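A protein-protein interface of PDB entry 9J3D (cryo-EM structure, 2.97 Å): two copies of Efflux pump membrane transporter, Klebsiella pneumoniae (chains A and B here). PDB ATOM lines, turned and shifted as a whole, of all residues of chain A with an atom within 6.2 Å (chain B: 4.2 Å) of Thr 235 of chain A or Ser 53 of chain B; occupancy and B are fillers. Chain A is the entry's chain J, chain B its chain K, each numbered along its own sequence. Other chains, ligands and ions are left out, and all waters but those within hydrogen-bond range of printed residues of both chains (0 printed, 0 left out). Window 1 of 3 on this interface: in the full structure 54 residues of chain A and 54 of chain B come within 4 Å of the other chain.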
ATOM      1  N   PRO A 217      -9.133  13.055 -12.282  1.00  0.00           N
ATOM      2  CA  PRO A 217      -9.706  12.641 -10.997  1.00  0.00           C
ATOM      3  C   PRO A 217     -10.880  13.519 -10.610  1.00  0.00           C
ATOM      4  O   PRO A 217     -10.747  14.419  -9.776  1.00  0.00           O
ATOM      5  CB  PRO A 217      -8.532  12.800 -10.029  1.00  0.00           C
ATOM      6  CG  PRO A 217      -7.742  13.919 -10.606  1.00  0.00           C
ATOM      7  CD  PRO A 217      -7.909  13.854 -12.108  1.00  0.00           C
ATOM      8  N   ALA A 218     -12.036  13.268 -11.217  1.00  0.00           N
ATOM      9  CA  ALA A 218     -13.175  14.169 -11.049  1.00  0.00           C
ATOM     10  C   ALA A 218     -13.719  14.145  -9.628  1.00  0.00           C
ATOM     11  O   ALA A 218     -13.728  15.167  -8.938  1.00  0.00           O
ATOM     12  CB  ALA A 218     -14.288  13.801 -12.020  1.00  0.00           C
ATOM     13  N   GLY A 219     -14.212  12.990  -9.195  1.00  0.00           N
ATOM     14  CA  GLY A 219     -14.763  12.881  -7.862  1.00  0.00           C
ATOM     15  C   GLY A 219     -16.179  12.351  -7.831  1.00  0.00           C
ATOM     16  O   GLY A 219     -16.585  11.583  -8.707  1.00  0.00           O
ATOM     17  N   ALA A 220     -16.944  12.758  -6.822  1.00  0.00           N
ATOM     18  CA  ALA A 220     -18.302  12.279  -6.638  1.00  0.00           C
ATOM     19  C   ALA A 220     -19.149  13.379  -6.022  1.00  0.00           C
ATOM     20  O   ALA A 220     -18.698  14.080  -5.114  1.00  0.00           O
ATOM     21  CB  ALA A 220     -18.331  11.034  -5.745  1.00  0.00           C
ATOM     22  N   PHE A 221     -20.377  13.524  -6.516  1.00  0.00           N
ATOM     23  CA  PHE A 221     -21.299  14.500  -5.958  1.00  0.00           C
ATOM     24  C   PHE A 221     -21.963  13.926  -4.710  1.00  0.00           C
ATOM     25  O   PHE A 221     -22.004  12.713  -4.497  1.00  0.00           O
ATOM     26  CB  PHE A 221     -22.325  14.926  -7.004  1.00  0.00           C
ATOM     27  CG  PHE A 221     -23.442  13.941  -7.213  1.00  0.00           C
ATOM     28  CD1 PHE A 221     -24.599  14.007  -6.460  1.00  0.00           C
ATOM     29  CD2 PHE A 221     -23.341  12.960  -8.180  1.00  0.00           C
ATOM     30  CE1 PHE A 221     -25.623  13.105  -6.659  1.00  0.00           C
ATOM     31  CE2 PHE A 221     -24.365  12.057  -8.382  1.00  0.00           C
ATOM     32  CZ  PHE A 221     -25.506  12.132  -7.622  1.00  0.00           C
ATOM     33  N   THR A 233     -24.800   9.860  -3.018  1.00  0.00           N
ATOM     34  CA  THR A 233     -23.389   9.977  -3.382  1.00  0.00           C
ATOM     35  C   THR A 233     -23.029   9.001  -4.499  1.00  0.00           C
ATOM     36  O   THR A 233     -23.259   7.796  -4.385  1.00  0.00           O
ATOM     37  CB  THR A 233     -22.500   9.732  -2.161  1.00  0.00           C
ATOM     38  OG1 THR A 233     -21.165   9.445  -2.591  1.00  0.00           O
ATOM     39  CG2 THR A 233     -23.023   8.573  -1.338  1.00  0.00           C
ATOM     40  N   ALA A 234     -22.471   9.532  -5.587  1.00  0.00           N
ATOM     41  CA  ALA A 234     -22.179   8.726  -6.764  1.00  0.00           C
ATOM     42  C   ALA A 234     -21.013   9.332  -7.533  1.00  0.00           C
ATOM     43  O   ALA A 234     -20.836  10.552  -7.542  1.00  0.00           O
ATOM     44  CB  ALA A 234     -23.403   8.611  -7.674  1.00  0.00           C
ATOM     45  N   THR A 235     -20.246   8.472  -8.200  1.00  0.00           N
ATOM     46  CA  THR A 235     -18.992   8.884  -8.817  1.00  0.00           C
ATOM     47  C   THR A 235     -19.244   9.652 -10.111  1.00  0.00           C
ATOM     48  O   THR A 235     -20.325   9.559 -10.699  1.00  0.00           O
ATOM     49  CB  THR A 235     -18.126   7.656  -9.090  1.00  0.00           C
ATOM     50  OG1 THR A 235     -18.259   6.733  -8.003  1.00  0.00           O
ATOM     51  CG2 THR A 235     -16.666   8.042  -9.214  1.00  0.00           C
ATOM     52  N   LEU A 236     -18.235  10.411 -10.556  1.00  0.00           N
ATOM     53  CA  LEU A 236     -18.367  11.223 -11.762  1.00  0.00           C
ATOM     54  C   LEU A 236     -17.618  10.615 -12.948  1.00  0.00           C
ATOM     55  O   LEU A 236     -17.991  10.852 -14.101  1.00  0.00           O
ATOM     56  CB  LEU A 236     -17.881  12.645 -11.488  1.00  0.00           C
ATOM     57  CG  LEU A 236     -18.756  13.443 -10.524  1.00  0.00           C
ATOM     58  CD1 LEU A 236     -18.287  14.882 -10.435  1.00  0.00           C
ATOM     59  CD2 LEU A 236     -20.214  13.377 -10.942  1.00  0.00           C
ATOM     60  N   THR A 237     -16.547   9.861 -12.686  1.00  0.00           N
ATOM     61  CA  THR A 237     -15.918   8.958 -13.652  1.00  0.00           C
ATOM     62  C   THR A 237     -15.730   9.529 -15.065  1.00  0.00           C
ATOM     63  O   THR A 237     -16.274   9.016 -16.046  1.00  0.00           O
ATOM     64  CB  THR A 237     -16.688   7.617 -13.657  1.00  0.00           C
ATOM     65  OG1 THR A 237     -15.875   6.581 -14.226  1.00  0.00           O
ATOM     66  CG2 THR A 237     -18.077   7.674 -14.319  1.00  0.00           C
ATOM     67  N   GLY B  51     -10.209  12.571  -4.828  1.00  0.00           N
ATOM     68  CA  GLY B  51     -11.086  12.771  -5.959  1.00  0.00           C
ATOM     69  C   GLY B  51     -11.021  11.705  -7.029  1.00  0.00           C
ATOM     70  O   GLY B  51     -11.757  11.803  -8.019  1.00  0.00           O
ATOM     71  N   ALA B  52     -10.176  10.693  -6.871  1.00  0.00           N
ATOM     72  CA  ALA B  52     -10.056   9.651  -7.877  1.00  0.00           C
ATOM     73  C   ALA B  52     -11.008   8.504  -7.571  1.00  0.00           C
ATOM     74  O   ALA B  52     -11.168   8.099  -6.417  1.00  0.00           O
ATOM     75  CB  ALA B  52      -8.621   9.135  -7.947  1.00  0.00           C
ATOM     76  N   SER B  53     -11.642   7.982  -8.616  1.00  0.00           N
ATOM     77  CA  SER B  53     -12.539   6.852  -8.450  1.00  0.00           C
ATOM     78  C   SER B  53     -11.747   5.584  -8.145  1.00  0.00           C
ATOM     79  O   SER B  53     -10.517   5.545  -8.243  1.00  0.00           O
ATOM     80  CB  SER B  53     -13.387   6.647  -9.704  1.00  0.00           C
ATOM     81  OG  SER B  53     -12.621   6.085 -10.753  1.00  0.00           O
ATOM     82  N   ALA B  54     -12.476   4.533  -7.767  1.00  0.00           N
ATOM     83  CA  ALA B  54     -11.830   3.269  -7.434  1.00  0.00           C
ATOM     84  C   ALA B  54     -11.085   2.692  -8.627  1.00  0.00           C
ATOM     85  O   ALA B  54      -9.962   2.197  -8.486  1.00  0.00           O
ATOM     86  CB  ALA B  54     -12.867   2.271  -6.925  1.00  0.00           C
ATOM     87  N   GLN B  55     -11.690   2.746  -9.813  1.00  0.00           N
ATOM     88  CA  GLN B  55     -11.042   2.184 -10.992  1.00  0.00           C
ATOM     89  C   GLN B  55      -9.870   3.046 -11.439  1.00  0.00           C
ATOM     90  O   GLN B  55      -8.842   2.528 -11.889  1.00  0.00           O
ATOM     91  CB  GLN B  55     -12.059   2.025 -12.122  1.00  0.00           C
ATOM     92  CG  GLN B  55     -11.543   1.289 -13.356  1.00  0.00           C
ATOM     93  CD  GLN B  55     -10.645   0.108 -13.027  1.00  0.00           C
ATOM     94  OE1 GLN B  55     -11.117  -1.019 -12.876  1.00  0.00           O
ATOM     95  NE2 GLN B  55      -9.342   0.354 -12.952  1.00  0.00           N
ATOM     96  N   VAL B  56     -10.012   4.370 -11.335  1.00  0.00           N
ATOM     97  CA  VAL B  56      -8.918   5.263 -11.705  1.00  0.00           C
ATOM     98  C   VAL B  56      -7.724   5.049 -10.786  1.00  0.00           C
ATOM     99  O   VAL B  56      -6.579   4.958 -11.243  1.00  0.00           O
ATOM    100  CB  VAL B  56      -9.391   6.727 -11.689  1.00  0.00           C
ATOM    101  CG1 VAL B  56      -8.208   7.669 -11.798  1.00  0.00           C
ATOM    102  CG2 VAL B  56     -10.367   6.974 -12.825  1.00  0.00           C
ATOM    103  N   LEU B  57      -7.971   4.956  -9.479  1.00  0.00           N
ATOM    104  CA  LEU B  57      -6.902   4.617  -8.548  1.00  0.00           C
ATOM    105  C   LEU B  57      -6.327   3.242  -8.853  1.00  0.00           C
ATOM    106  O   LEU B  57      -5.116   3.023  -8.738  1.00  0.00           O
ATOM    107  CB  LEU B  57      -7.424   4.665  -7.115  1.00  0.00           C
ATOM    108  CG  LEU B  57      -6.371   4.643  -6.011  1.00  0.00           C
ATOM    109  CD1 LEU B  57      -5.170   5.468  -6.400  1.00  0.00           C
ATOM    110  CD2 LEU B  57      -6.953   5.129  -4.712  1.00  0.00           C
ATOM    111  N   PRO B 721     -23.928   2.801  -8.797  1.00  0.00           N
ATOM    112  CA  PRO B 721     -24.132   3.672  -9.960  1.00  0.00           C
ATOM    113  C   PRO B 721     -23.059   4.740 -10.088  1.00  0.00           C
ATOM    114  O   PRO B 721     -22.595   5.297  -9.089  1.00  0.00           O
ATOM    115  CB  PRO B 721     -25.508   4.292  -9.696  1.00  0.00           C
ATOM    116  CG  PRO B 721     -26.194   3.319  -8.808  1.00  0.00           C
ATOM    117  CD  PRO B 721     -25.123   2.740  -7.938  1.00  0.00           C
ATOM    118  N   GLN B 722     -22.670   5.031 -11.323  1.00  0.00           N
ATOM    119  CA  GLN B 722     -21.717   6.078 -11.647  1.00  0.00           C
ATOM    120  C   GLN B 722     -22.334   7.004 -12.685  1.00  0.00           C
ATOM    121  O   GLN B 722     -23.198   6.588 -13.463  1.00  0.00           O
ATOM    122  CB  GLN B 722     -20.407   5.491 -12.177  1.00  0.00           C
ATOM    123  CG  GLN B 722     -19.702   4.565 -11.201  1.00  0.00           C
ATOM    124  CD  GLN B 722     -18.380   4.059 -11.734  1.00  0.00           C
ATOM    125  OE1 GLN B 722     -18.006   4.342 -12.871  1.00  0.00           O
ATOM    126  NE2 GLN B 722     -17.659   3.310 -10.909  1.00  0.00           N
ATOM    127  N   LEU B 723     -21.898   8.260 -12.686  1.00  0.00           N
ATOM    128  CA  LEU B 723     -22.445   9.270 -13.589  1.00  0.00           C
ATOM    129  C   LEU B 723     -21.374   9.647 -14.603  1.00  0.00           C
ATOM    130  O   LEU B 723     -20.635  10.612 -14.411  1.00  0.00           O
ATOM    131  CB  LEU B 723     -22.921  10.486 -12.804  1.00  0.00           C
ATOM    132  CG  LEU B 723     -23.578  11.601 -13.614  1.00  0.00           C
ATOM    133  CD1 LEU B 723     -24.915  11.142 -14.153  1.00  0.00           C
ATOM    134  CD2 LEU B 723     -23.742  12.851 -12.768  1.00  0.00           C
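O of Leu 236 of chain A sits close to O of Leu 723 of chain B (2.7 Å). The backbone NH (N) of Gly 219 of chain A sits at hydrogen-bond distance from the backbone carbonyl oxygen (O) of Gly 51 of chain B, 3.0 Å away. The side-chain hydroxyl of Thr 237 of chain A is in hydrogen-bond range of the side-chain amide oxygen of Gln 722 of chain B (3.4 Å). The backbone carbonyl oxygen (O) of Thr 235 of chain A sits at hydrogen-bond distance from the backbone NH (N) of Leu 723 of chain B (2.8 Å). O of Pro 217 of chain A sits close to O of Gly 51 of chain B (3.3 Å).
OG of Ser 53 of chain B sits at hydrogen-bond distance from N of Val 56 of chain B. N of Phe 221 of chain A sits at hydrogen-bond distance from O of Ala 234 of chain A. The backbone NH (N) of Leu 236 of chain A lies within hydrogen-bond range of the backbone carbonyl oxygen (O) of Gly 219 of chain A (2.7 Å).
Among the printed residues, pairs that only touch across the chains: Ala 218 of chain A with Gly 51 of chain B, Ala 234 of chain A with Pro 721 of chain B, Thr 235 of chain A with Ser 53 of chain B, Thr 235 of chain A with Gln 722 of chain B and Thr 237 of chain A with Leu 723 of chain B.
Of chain A, only Thr 235 comes within 4 Å of Ser 53 of chain B. Of the printed residues of chain B, Gly 219 of chain A touches Gly 51. Of the printed residues of chain B, Ala 234 of chain A touches Pro 721 (3.7 Å). Ala 54 of chain B touches none of the printed residues of chain A. Val 56 of chain B touches none of the printed residues of chain A. The nearest printed residue of chain B that does not touch Pro 217 of chain A is Ala 52 of chain B (4.1 Å).
Printed residues of chain B that touch a printed residue of chain A: Gly 51, Ser 53, Pro 721, Gln 722 and Leu 723. Hydrophobic or aromatic side chains of chain B within 4 Å of the printed part of chain A: Leu 723. Along chain A the printed residues that touch a printed residue of chain B span positions 217 to 237. Among the printed residues, no Asp or Glu carboxylate lies within 4 Å of a Lys or Arg side-chain nitrogen of the other chain.
No position is printed for both chains.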
